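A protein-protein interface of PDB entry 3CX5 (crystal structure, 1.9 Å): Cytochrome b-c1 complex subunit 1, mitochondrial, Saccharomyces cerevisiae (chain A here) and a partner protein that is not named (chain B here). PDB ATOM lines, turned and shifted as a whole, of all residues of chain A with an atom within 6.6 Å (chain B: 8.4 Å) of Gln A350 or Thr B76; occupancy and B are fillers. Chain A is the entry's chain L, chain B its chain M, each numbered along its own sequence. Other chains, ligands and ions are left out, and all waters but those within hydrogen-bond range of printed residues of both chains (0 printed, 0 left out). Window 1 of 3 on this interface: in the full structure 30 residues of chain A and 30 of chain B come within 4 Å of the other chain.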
ATOM      1  N   LEU A 343      -6.498  -4.351 -24.120  1.00  0.00           N
ATOM      2  CA  LEU A 343      -6.213  -3.079 -24.770  1.00  0.00           C
ATOM      3  C   LEU A 343      -7.215  -1.994 -24.375  1.00  0.00           C
ATOM      4  O   LEU A 343      -6.840  -0.830 -24.247  1.00  0.00           O
ATOM      5  CB  LEU A 343      -6.127  -3.251 -26.289  1.00  0.00           C
ATOM      6  CG  LEU A 343      -4.888  -4.013 -26.793  1.00  0.00           C
ATOM      7  CD1 LEU A 343      -4.932  -4.137 -28.313  1.00  0.00           C
ATOM      8  CD2 LEU A 343      -3.607  -3.296 -26.366  1.00  0.00           C
ATOM      9  N   LYS A 345      -8.680  -1.757 -21.444  1.00  0.00           N
ATOM     10  CA  LYS A 345      -8.267  -1.349 -20.098  1.00  0.00           C
ATOM     11  C   LYS A 345      -7.105  -0.370 -20.211  1.00  0.00           C
ATOM     12  O   LYS A 345      -7.054   0.639 -19.508  1.00  0.00           O
ATOM     13  CB  LYS A 345      -7.821  -2.556 -19.277  1.00  0.00           C
ATOM     14  CG  LYS A 345      -8.919  -3.530 -18.902  1.00  0.00           C
ATOM     15  CD  LYS A 345      -8.317  -4.684 -18.116  1.00  0.00           C
ATOM     16  CE  LYS A 345      -9.312  -5.797 -17.912  1.00  0.00           C
ATOM     17  NZ  LYS A 345      -8.730  -6.901 -17.091  1.00  0.00           N
ATOM     18  N   LEU A 346      -6.184  -0.660 -21.123  1.00  0.00           N
ATOM     19  CA  LEU A 346      -5.032   0.203 -21.339  1.00  0.00           C
ATOM     20  C   LEU A 346      -5.424   1.591 -21.865  1.00  0.00           C
ATOM     21  O   LEU A 346      -4.845   2.594 -21.443  1.00  0.00           O
ATOM     22  CB  LEU A 346      -4.039  -0.463 -22.294  1.00  0.00           C
ATOM     23  CG  LEU A 346      -2.743   0.295 -22.580  1.00  0.00           C
ATOM     24  CD1 LEU A 346      -1.933   0.459 -21.294  1.00  0.00           C
ATOM     25  CD2 LEU A 346      -1.935  -0.449 -23.633  1.00  0.00           C
ATOM     26  N   GLN A 347      -6.399   1.656 -22.774  1.00  0.00           N
ATOM     27  CA  GLN A 347      -6.828   2.946 -23.324  1.00  0.00           C
ATOM     28  C   GLN A 347      -7.588   3.754 -22.274  1.00  0.00           C
ATOM     29  O   GLN A 347      -7.391   4.963 -22.155  1.00  0.00           O
ATOM     30  CB  GLN A 347      -7.671   2.782 -24.608  1.00  0.00           C
ATOM     31  CG  GLN A 347      -9.189   2.793 -24.413  1.00  0.00           C
ATOM     32  CD  GLN A 347      -9.972   3.057 -25.699  1.00  0.00           C
ATOM     33  OE1 GLN A 347     -10.601   4.104 -25.850  1.00  0.00           O
ATOM     34  NE2 GLN A 347      -9.960   2.092 -26.614  1.00  0.00           N
ATOM     35  N   LEU A 348      -8.453   3.076 -21.519  1.00  0.00           N
ATOM     36  CA  LEU A 348      -9.228   3.717 -20.460  1.00  0.00           C
ATOM     37  C   LEU A 348      -8.271   4.236 -19.393  1.00  0.00           C
ATOM     38  O   LEU A 348      -8.439   5.343 -18.878  1.00  0.00           O
ATOM     39  CB  LEU A 348     -10.214   2.721 -19.848  1.00  0.00           C
ATOM     40  CG  LEU A 348     -11.695   2.930 -20.185  1.00  0.00           C
ATOM     41  CD1 LEU A 348     -11.879   3.260 -21.655  1.00  0.00           C
ATOM     42  CD2 LEU A 348     -12.490   1.699 -19.797  1.00  0.00           C
ATOM     43  N   GLY A 349      -7.248   3.440 -19.092  1.00  0.00           N
ATOM     44  CA  GLY A 349      -6.259   3.836 -18.109  1.00  0.00           C
ATOM     45  C   GLY A 349      -5.511   5.084 -18.543  1.00  0.00           C
ATOM     46  O   GLY A 349      -5.304   5.992 -17.746  1.00  0.00           O
ATOM     47  N   GLN A 350      -5.123   5.147 -19.813  1.00  0.00           N
ATOM     48  CA  GLN A 350      -4.401   6.309 -20.322  1.00  0.00           C
ATOM     49  C   GLN A 350      -5.277   7.558 -20.419  1.00  0.00           C
ATOM     50  O   GLN A 350      -4.776   8.684 -20.334  1.00  0.00           O
ATOM     51  CB  GLN A 350      -3.768   5.994 -21.679  1.00  0.00           C
ATOM     52  CG  GLN A 350      -2.657   4.953 -21.602  1.00  0.00           C
ATOM     53  CD  GLN A 350      -2.005   4.691 -22.946  1.00  0.00           C
ATOM     54  OE1 GLN A 350      -2.599   4.067 -23.827  1.00  0.00           O
ATOM     55  NE2 GLN A 350      -0.776   5.172 -23.110  1.00  0.00           N
ATOM     56  N   LEU A 351      -6.580   7.354 -20.593  1.00  0.00           N
ATOM     57  CA  LEU A 351      -7.524   8.465 -20.695  1.00  0.00           C
ATOM     58  C   LEU A 351      -7.847   9.043 -19.315  1.00  0.00           C
ATOM     59  O   LEU A 351      -7.897  10.262 -19.138  1.00  0.00           O
ATOM     60  CB  LEU A 351      -8.820   8.008 -21.375  1.00  0.00           C
ATOM     61  CG  LEU A 351      -9.935   9.048 -21.544  1.00  0.00           C
ATOM     62  CD1 LEU A 351      -9.505  10.122 -22.543  1.00  0.00           C
ATOM     63  CD2 LEU A 351     -11.214   8.366 -22.017  1.00  0.00           C
ATOM     64  N   TYR A 352      -8.064   8.158 -18.348  1.00  0.00           N
ATOM     65  CA  TYR A 352      -8.406   8.569 -16.990  1.00  0.00           C
ATOM     66  C   TYR A 352      -7.232   8.776 -16.039  1.00  0.00           C
ATOM     67  O   TYR A 352      -7.341   9.541 -15.082  1.00  0.00           O
ATOM     68  CB  TYR A 352      -9.415   7.592 -16.384  1.00  0.00           C
ATOM     69  CG  TYR A 352     -10.769   7.680 -17.038  1.00  0.00           C
ATOM     70  CD1 TYR A 352     -11.588   8.790 -16.832  1.00  0.00           C
ATOM     71  CD2 TYR A 352     -11.224   6.675 -17.886  1.00  0.00           C
ATOM     72  CE1 TYR A 352     -12.822   8.897 -17.453  1.00  0.00           C
ATOM     73  CE2 TYR A 352     -12.463   6.773 -18.516  1.00  0.00           C
ATOM     74  CZ  TYR A 352     -13.254   7.888 -18.295  1.00  0.00           C
ATOM     75  OH  TYR A 352     -14.475   8.001 -18.913  1.00  0.00           O
ATOM     76  N   GLU A 353      -6.118   8.098 -16.292  1.00  0.00           N
ATOM     77  CA  GLU A 353      -4.951   8.234 -15.432  1.00  0.00           C
ATOM     78  C   GLU A 353      -3.833   8.978 -16.126  1.00  0.00           C
ATOM     79  O   GLU A 353      -2.701   8.508 -16.216  1.00  0.00           O
ATOM     80  CB  GLU A 353      -4.478   6.876 -14.928  1.00  0.00           C
ATOM     81  CG  GLU A 353      -5.530   6.155 -14.105  1.00  0.00           C
ATOM     82  CD  GLU A 353      -5.051   4.829 -13.562  1.00  0.00           C
ATOM     83  OE1 GLU A 353      -4.017   4.317 -14.044  1.00  0.00           O
ATOM     84  OE2 GLU A 353      -5.714   4.295 -12.645  1.00  0.00           O
ATOM     85  N   SER A 354      -4.197  10.127 -16.675  1.00  0.00           N
ATOM     86  CA  SER A 354      -3.262  11.008 -17.346  1.00  0.00           C
ATOM     87  C   SER A 354      -2.639  11.855 -16.230  1.00  0.00           C
ATOM     88  O   SER A 354      -3.160  11.905 -15.108  1.00  0.00           O
ATOM     89  CB  SER A 354      -4.029  11.903 -18.323  1.00  0.00           C
ATOM     90  OG  SER A 354      -3.197  12.904 -18.876  1.00  0.00           O
ATOM     91  N   GLY A 355      -1.509  12.488 -16.512  1.00  0.00           N
ATOM     92  CA  GLY A 355      -0.896  13.327 -15.495  1.00  0.00           C
ATOM     93  C   GLY A 355      -1.318  14.774 -15.682  1.00  0.00           C
ATOM     94  O   GLY A 355      -0.703  15.686 -15.126  1.00  0.00           O
ATOM     95  N   LEU A 377     -12.402   3.636 -12.250  1.00  0.00           N
ATOM     96  CA  LEU A 377     -11.707   2.832 -13.241  1.00  0.00           C
ATOM     97  C   LEU A 377     -11.789   1.365 -12.827  1.00  0.00           C
ATOM     98  O   LEU A 377     -11.836   0.472 -13.675  1.00  0.00           O
ATOM     99  CB  LEU A 377     -10.252   3.285 -13.360  1.00  0.00           C
ATOM    100  CG  LEU A 377      -9.538   2.922 -14.662  1.00  0.00           C
ATOM    101  CD1 LEU A 377     -10.352   3.398 -15.857  1.00  0.00           C
ATOM    102  CD2 LEU A 377      -8.158   3.544 -14.676  1.00  0.00           C
ATOM    103  N   LYS B  11      -3.951   2.088 -11.901  1.00  0.00           N
ATOM    104  CA  LYS B  11      -4.046   0.806 -12.588  1.00  0.00           C
ATOM    105  C   LYS B  11      -3.059   0.694 -13.743  1.00  0.00           C
ATOM    106  O   LYS B  11      -2.739  -0.410 -14.193  1.00  0.00           O
ATOM    107  CB  LYS B  11      -5.480   0.558 -13.050  1.00  0.00           C
ATOM    108  CG  LYS B  11      -6.402   0.296 -11.875  1.00  0.00           C
ATOM    109  CD  LYS B  11      -7.783  -0.126 -12.292  1.00  0.00           C
ATOM    110  CE  LYS B  11      -8.584  -0.569 -11.081  1.00  0.00           C
ATOM    111  NZ  LYS B  11      -7.970  -1.748 -10.401  1.00  0.00           N
ATOM    112  N   ILE B  12      -2.529   1.840 -14.161  1.00  0.00           N
ATOM    113  CA  ILE B  12      -1.567   1.922 -15.257  1.00  0.00           C
ATOM    114  C   ILE B  12      -0.223   2.456 -14.774  1.00  0.00           C
ATOM    115  O   ILE B  12      -0.164   3.333 -13.912  1.00  0.00           O
ATOM    116  CB  ILE B  12      -2.110   2.838 -16.401  1.00  0.00           C
ATOM    117  CG1 ILE B  12      -3.257   2.143 -17.127  1.00  0.00           C
ATOM    118  CG2 ILE B  12      -1.013   3.201 -17.390  1.00  0.00           C
ATOM    119  CD1 ILE B  12      -2.863   0.844 -17.772  1.00  0.00           C
ATOM    120  N   SER B  13       0.852   1.932 -15.353  1.00  0.00           N
ATOM    121  CA  SER B  13       2.205   2.347 -15.009  1.00  0.00           C
ATOM    122  C   SER B  13       3.021   2.560 -16.277  1.00  0.00           C
ATOM    123  O   SER B  13       2.693   2.020 -17.339  1.00  0.00           O
ATOM    124  CB  SER B  13       2.890   1.273 -14.160  1.00  0.00           C
ATOM    125  OG  SER B  13       2.127   0.961 -13.011  1.00  0.00           O
ATOM    126  N   THR B  14       4.062   3.380 -16.170  1.00  0.00           N
ATOM    127  CA  THR B  14       4.950   3.633 -17.296  1.00  0.00           C
ATOM    128  C   THR B  14       6.376   3.364 -16.840  1.00  0.00           C
ATOM    129  O   THR B  14       6.737   3.644 -15.699  1.00  0.00           O
ATOM    130  CB  THR B  14       4.841   5.080 -17.840  1.00  0.00           C
ATOM    131  OG1 THR B  14       5.274   6.009 -16.841  1.00  0.00           O
ATOM    132  CG2 THR B  14       3.409   5.397 -18.246  1.00  0.00           C
ATOM    133  N   LEU B  15       7.170   2.785 -17.731  1.00  0.00           N
ATOM    134  CA  LEU B  15       8.554   2.463 -17.436  1.00  0.00           C
ATOM    135  C   LEU B  15       9.378   3.112 -18.529  1.00  0.00           C
ATOM    136  O   LEU B  15       9.032   3.020 -19.704  1.00  0.00           O
ATOM    137  CB  LEU B  15       8.747   0.943 -17.449  1.00  0.00           C
ATOM    138  CG  LEU B  15       9.928   0.325 -16.689  1.00  0.00           C
ATOM    139  CD1 LEU B  15      11.239   0.578 -17.396  1.00  0.00           C
ATOM    140  CD2 LEU B  15       9.970   0.883 -15.274  1.00  0.00           C
ATOM    141  N   ALA B  16      10.452   3.788 -18.139  1.00  0.00           N
ATOM    142  CA  ALA B  16      11.314   4.458 -19.097  1.00  0.00           C
ATOM    143  C   ALA B  16      12.786   4.166 -18.858  1.00  0.00           C
ATOM    144  O   ALA B  16      13.265   4.202 -17.724  1.00  0.00           O
ATOM    145  CB  ALA B  16      11.074   5.959 -19.054  1.00  0.00           C
ATOM    146  N   SER B  55       2.422  -8.570 -25.633  1.00  0.00           N
ATOM    147  CA  SER B  55       2.114  -7.333 -24.926  1.00  0.00           C
ATOM    148  C   SER B  55       0.669  -6.862 -25.079  1.00  0.00           C
ATOM    149  O   SER B  55       0.121  -6.259 -24.155  1.00  0.00           O
ATOM    150  CB  SER B  55       3.106  -6.217 -25.276  1.00  0.00           C
ATOM    151  OG  SER B  55       3.315  -6.107 -26.669  1.00  0.00           O
ATOM    152  N   LEU B  58      -1.513  -8.963 -22.531  1.00  0.00           N
ATOM    153  CA  LEU B  58      -1.479  -8.564 -21.126  1.00  0.00           C
ATOM    154  C   LEU B  58      -1.829  -7.090 -20.927  1.00  0.00           C
ATOM    155  O   LEU B  58      -2.031  -6.643 -19.802  1.00  0.00           O
ATOM    156  CB  LEU B  58      -0.166  -8.948 -20.423  1.00  0.00           C
ATOM    157  CG  LEU B  58       1.133  -9.261 -21.161  1.00  0.00           C
ATOM    158  CD1 LEU B  58       1.674  -8.011 -21.774  1.00  0.00           C
ATOM    159  CD2 LEU B  58       2.148  -9.819 -20.187  1.00  0.00           C
ATOM    160  N   GLY B  59      -1.948  -6.359 -22.035  1.00  0.00           N
ATOM    161  CA  GLY B  59      -2.317  -4.956 -21.978  1.00  0.00           C
ATOM    162  C   GLY B  59      -1.200  -3.943 -21.840  1.00  0.00           C
ATOM    163  O   GLY B  59      -1.175  -3.189 -20.871  1.00  0.00           O
ATOM    164  N   GLY B  60      -0.314  -3.881 -22.829  1.00  0.00           N
ATOM    165  CA  GLY B  60       0.782  -2.930 -22.786  1.00  0.00           C
ATOM    166  C   GLY B  60       1.295  -2.559 -24.166  1.00  0.00           C
ATOM    167  O   GLY B  60       1.068  -3.290 -25.131  1.00  0.00           O
ATOM    168  N   THR B  61       1.977  -1.418 -24.258  1.00  0.00           N
ATOM    169  CA  THR B  61       2.538  -0.932 -25.519  1.00  0.00           C
ATOM    170  C   THR B  61       3.958  -0.410 -25.339  1.00  0.00           C
ATOM    171  O   THR B  61       4.331   0.059 -24.262  1.00  0.00           O
ATOM    172  CB  THR B  61       1.680   0.197 -26.152  1.00  0.00           C
ATOM    173  OG1 THR B  61       1.454   1.232 -25.187  1.00  0.00           O
ATOM    174  CG2 THR B  61       0.344  -0.346 -26.653  1.00  0.00           C
ATOM    175  N   PHE B  62       4.734  -0.470 -26.419  1.00  0.00           N
ATOM    176  CA  PHE B  62       6.128  -0.033 -26.420  1.00  0.00           C
ATOM    177  C   PHE B  62       6.369   1.088 -27.422  1.00  0.00           C
ATOM    178  O   PHE B  62       5.699   1.164 -28.456  1.00  0.00           O
ATOM    179  CB  PHE B  62       7.046  -1.203 -26.777  1.00  0.00           C
ATOM    180  CG  PHE B  62       7.030  -2.319 -25.778  1.00  0.00           C
ATOM    181  CD1 PHE B  62       6.329  -3.490 -26.039  1.00  0.00           C
ATOM    182  CD2 PHE B  62       7.746  -2.214 -24.585  1.00  0.00           C
ATOM    183  CE1 PHE B  62       6.340  -4.545 -25.128  1.00  0.00           C
ATOM    184  CE2 PHE B  62       7.763  -3.265 -23.666  1.00  0.00           C
ATOM    185  CZ  PHE B  62       7.058  -4.434 -23.940  1.00  0.00           C
ATOM    186  N   LYS B  63       7.382   1.904 -27.143  1.00  0.00           N
ATOM    187  CA  LYS B  63       7.750   3.022 -28.001  1.00  0.00           C
ATOM    188  C   LYS B  63       9.170   3.485 -27.690  1.00  0.00           C
ATOM    189  O   LYS B  63       9.586   3.496 -26.529  1.00  0.00           O
ATOM    190  CB  LYS B  63       6.770   4.186 -27.792  1.00  0.00           C
ATOM    191  CG  LYS B  63       7.148   5.495 -28.480  1.00  0.00           C
ATOM    192  CD  LYS B  63       7.258   5.334 -29.998  1.00  0.00           C
ATOM    193  CE  LYS B  63       7.645   6.646 -30.685  1.00  0.00           C
ATOM    194  NZ  LYS B  63       7.777   6.474 -32.166  1.00  0.00           N
ATOM    195  N   LEU B  73      13.380   4.442 -24.279  1.00  0.00           N
ATOM    196  CA  LEU B  73      12.551   3.271 -24.505  1.00  0.00           C
ATOM    197  C   LEU B  73      11.480   3.320 -23.428  1.00  0.00           C
ATOM    198  O   LEU B  73      11.781   3.246 -22.238  1.00  0.00           O
ATOM    199  CB  LEU B  73      13.373   1.984 -24.403  1.00  0.00           C
ATOM    200  CG  LEU B  73      14.492   1.844 -25.439  1.00  0.00           C
ATOM    201  CD1 LEU B  73      15.693   2.688 -25.024  1.00  0.00           C
ATOM    202  CD2 LEU B  73      14.893   0.388 -25.574  1.00  0.00           C
ATOM    203  N   LYS B  74      10.231   3.473 -23.851  1.00  0.00           N
ATOM    204  CA  LYS B  74       9.118   3.573 -22.922  1.00  0.00           C
ATOM    205  C   LYS B  74       8.089   2.460 -23.061  1.00  0.00           C
ATOM    206  O   LYS B  74       7.820   1.969 -24.158  1.00  0.00           O
ATOM    207  CB  LYS B  74       8.435   4.935 -23.085  1.00  0.00           C
ATOM    208  CG  LYS B  74       7.310   5.209 -22.096  1.00  0.00           C
ATOM    209  CD  LYS B  74       6.695   6.592 -22.308  1.00  0.00           C
ATOM    210  CE  LYS B  74       5.605   6.868 -21.274  1.00  0.00           C
ATOM    211  NZ  LYS B  74       4.993   8.224 -21.419  1.00  0.00           N
ATOM    212  N   ALA B  75       7.524   2.069 -21.922  1.00  0.00           N
ATOM    213  CA  ALA B  75       6.497   1.042 -21.861  1.00  0.00           C
ATOM    214  C   ALA B  75       5.367   1.573 -20.987  1.00  0.00           C
ATOM    215  O   ALA B  75       5.612   2.248 -19.985  1.00  0.00           O
ATOM    216  CB  ALA B  75       7.060  -0.243 -21.281  1.00  0.00           C
ATOM    217  N   THR B  76       4.135   1.326 -21.417  1.00  0.00           N
ATOM    218  CA  THR B  76       2.943   1.755 -20.693  1.00  0.00           C
ATOM    219  C   THR B  76       2.141   0.473 -20.541  1.00  0.00           C
ATOM    220  O   THR B  76       1.844  -0.190 -21.531  1.00  0.00           O
ATOM    221  CB  THR B  76       2.158   2.797 -21.500  1.00  0.00           C
ATOM    222  OG1 THR B  76       3.051   3.841 -21.913  1.00  0.00           O
ATOM    223  CG2 THR B  76       1.048   3.399 -20.654  1.00  0.00           C
ATOM    224  N   PHE B  77       1.752   0.145 -19.313  1.00  0.00           N
ATOM    225  CA  PHE B  77       1.065  -1.119 -19.069  1.00  0.00           C
ATOM    226  C   PHE B  77       0.272  -1.183 -17.767  1.00  0.00           C
ATOM    227  O   PHE B  77       0.289  -0.250 -16.959  1.00  0.00           O
ATOM    228  CB  PHE B  77       2.133  -2.212 -19.012  1.00  0.00           C
ATOM    229  CG  PHE B  77       3.246  -1.902 -18.041  1.00  0.00           C
ATOM    230  CD1 PHE B  77       3.186  -2.351 -16.726  1.00  0.00           C
ATOM    231  CD2 PHE B  77       4.323  -1.106 -18.428  1.00  0.00           C
ATOM    232  CE1 PHE B  77       4.181  -2.005 -15.807  1.00  0.00           C
ATOM    233  CE2 PHE B  77       5.323  -0.754 -17.520  1.00  0.00           C
ATOM    234  CZ  PHE B  77       5.250  -1.204 -16.206  1.00  0.00           C
ATOM    235  N   LEU B  78      -0.390  -2.320 -17.567  1.00  0.00           N
ATOM    236  CA  LEU B  78      -1.158  -2.580 -16.356  1.00  0.00           C
ATOM    237  C   LEU B  78      -0.145  -2.834 -15.239  1.00  0.00           C
ATOM    238  O   LEU B  78       0.739  -3.688 -15.367  1.00  0.00           O
ATOM    239  CB  LEU B  78      -2.075  -3.791 -16.553  1.00  0.00           C
ATOM    240  CG  LEU B  78      -3.202  -3.564 -17.570  1.00  0.00           C
ATOM    241  CD1 LEU B  78      -4.001  -4.832 -17.779  1.00  0.00           C
ATOM    242  CD2 LEU B  78      -4.107  -2.441 -17.092  1.00  0.00           C
ATOM    243  N   LYS B  79      -0.273  -2.056 -14.168  1.00  0.00           N
ATOM    244  CA  LYS B  79       0.616  -2.091 -13.004  1.00  0.00           C
ATOM    245  C   LYS B  79       1.253  -3.416 -12.572  1.00  0.00           C
ATOM    246  O   LYS B  79       2.475  -3.495 -12.449  1.00  0.00           O
ATOM    247  CB  LYS B  79      -0.078  -1.419 -11.807  1.00  0.00           C
ATOM    248  CG  LYS B  79       0.809  -1.188 -10.578  1.00  0.00           C
ATOM    249  CD  LYS B  79       0.138  -0.233  -9.586  1.00  0.00           C
ATOM    250  CE  LYS B  79       0.902  -0.125  -8.265  1.00  0.00           C
ATOM    251  NZ  LYS B  79       2.269   0.453  -8.409  1.00  0.00           N
ATOM    252  N   ASP B  81       2.024  -6.042 -14.093  1.00  0.00           N
ATOM    253  CA  ASP B  81       2.876  -6.712 -15.074  1.00  0.00           C
ATOM    254  C   ASP B  81       4.293  -6.159 -15.192  1.00  0.00           C
ATOM    255  O   ASP B  81       5.029  -6.518 -16.111  1.00  0.00           O
ATOM    256  CB  ASP B  81       2.189  -6.712 -16.445  1.00  0.00           C
ATOM    257  CG  ASP B  81       0.893  -7.502 -16.445  1.00  0.00           C
ATOM    258  OD1 ASP B  81      -0.091  -7.053 -17.079  1.00  0.00           O
ATOM    259  OD2 ASP B  81       0.860  -8.576 -15.807  1.00  0.00           O
ATOM    260  N   TYR B  85       7.763  -6.156 -18.511  1.00  0.00           N
ATOM    261  CA  TYR B  85       8.236  -4.980 -19.225  1.00  0.00           C
ATOM    262  C   TYR B  85       9.666  -4.561 -18.923  1.00  0.00           C
ATOM    263  O   TYR B  85      10.339  -3.996 -19.786  1.00  0.00           O
ATOM    264  CB  TYR B  85       7.255  -3.829 -19.035  1.00  0.00           C
ATOM    265  CG  TYR B  85       5.914  -4.167 -19.633  1.00  0.00           C
ATOM    266  CD1 TYR B  85       4.950  -4.854 -18.894  1.00  0.00           C
ATOM    267  CD2 TYR B  85       5.633  -3.862 -20.964  1.00  0.00           C
ATOM    268  CE1 TYR B  85       3.740  -5.231 -19.472  1.00  0.00           C
ATOM    269  CE2 TYR B  85       4.433  -4.232 -21.548  1.00  0.00           C
ATOM    270  CZ  TYR B  85       3.491  -4.912 -20.800  1.00  0.00           C
ATOM    271  OH  TYR B  85       2.293  -5.251 -21.383  1.00  0.00           O
ATOM    272  N   LEU B  89      12.410  -4.421 -22.086  1.00  0.00           N
ATOM    273  CA  LEU B  89      13.262  -3.272 -22.367  1.00  0.00           C
ATOM    274  C   LEU B  89      14.732  -3.638 -22.221  1.00  0.00           C
ATOM    275  O   LEU B  89      15.573  -3.169 -22.988  1.00  0.00           O
ATOM    276  CB  LEU B  89      12.902  -2.100 -21.449  1.00  0.00           C
ATOM    277  CG  LEU B  89      11.512  -1.487 -21.665  1.00  0.00           C
ATOM    278  CD1 LEU B  89      11.207  -0.458 -20.595  1.00  0.00           C
ATOM    279  CD2 LEU B  89      11.437  -0.841 -23.031  1.00  0.00           C
ATOM    280  N   GLU B 174       6.931   5.407 -13.396  1.00  0.00           N
ATOM    281  CA  GLU B 174       5.841   6.256 -12.925  1.00  0.00           C
ATOM    282  C   GLU B 174       4.705   5.330 -12.505  1.00  0.00           C
ATOM    283  O   GLU B 174       4.356   4.399 -13.237  1.00  0.00           O
ATOM    284  CB  GLU B 174       5.385   7.216 -14.026  1.00  0.00           C
ATOM    285  CG  GLU B 174       4.884   8.570 -13.519  1.00  0.00           C
ATOM    286  CD  GLU B 174       6.013   9.518 -13.093  1.00  0.00           C
ATOM    287  OE1 GLU B 174       6.142  10.600 -13.709  1.00  0.00           O
ATOM    288  OE2 GLU B 174       6.762   9.194 -12.143  1.00  0.00           O
ATOM    289  N   ASN B 175       4.143   5.579 -11.322  1.00  0.00           N
ATOM    290  CA  ASN B 175       3.076   4.750 -10.756  1.00  0.00           C
ATOM    291  C   ASN B 175       3.663   3.362 -10.514  1.00  0.00           C
ATOM    292  O   ASN B 175       2.978   2.347 -10.640  1.00  0.00           O
ATOM    293  CB  ASN B 175       1.872   4.655 -11.706  1.00  0.00           C
ATOM    294  CG  ASN B 175       1.194   5.999 -11.944  1.00  0.00           C
ATOM    295  OD1 ASN B 175       1.423   6.970 -11.218  1.00  0.00           O
ATOM    296  ND2 ASN B 175       0.348   6.055 -12.968  1.00  0.00           N
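The side-chain carboxylate (OE2) of Glu A353 lies within hydrogen-bond range of the backbone NH (N) of Lys B11 (2.9 Å). The backbone NH (N) of Ile B12 sits at hydrogen-bond distance from the side-chain carboxylate (OE1) of Glu A353 (2.9 Å).
Thr B76 touches two residues of chain A. Of chain B, only Ile B12 (3.6 Å) comes within 4 Å of Gly A349. Of the printed residues of chain A, Gly B59 touches Leu A346. Printed residues of chain A within 4 Å of Ile B12: Leu A346, Gly A349 and Glu A353. The nearest printed residue of chain A that does not touch Thr B76 is Gly A349 (7.1 Å).
Hydrophobic or aromatic side chains of chain B that line the printed part of chain A: Ile B12. Of the 13 printed residues of chain A, 4 touch a printed residue of chain B.
N of Lys B79 lies within hydrogen-bond range of O of Lys B11 (3.0 Å). The backbone carbonyl oxygen of Ile B12 is in hydrogen-bond range of the side-chain amide nitrogen of Asn B175 (2.9 Å). The backbone NH (N) of Gly B60 is in hydrogen-bond range of the backbone carbonyl oxygen (O) of Ser B55 (2.8 Å). OH of Tyr B85 sits close to N of Gly B60 (3.3 Å). The backbone NH of Thr B61 is in hydrogen-bond range of the backbone carbonyl oxygen of Thr B76.
Among the printed residues, pairs that only touch across the chains: Gln A350 with Thr B76 (3.5 Å), Gly A349 with Ile B12 (3.6 Å), Leu A346 with Ile B12 (3.7 Å), Leu A346 with Gly B59 (3.7 Å), Leu A346 with Gly B60 (3.8 Å), Leu A346 with Thr B61 (3.8 Å) and Leu A346 with Thr B76 (3.8 Å).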
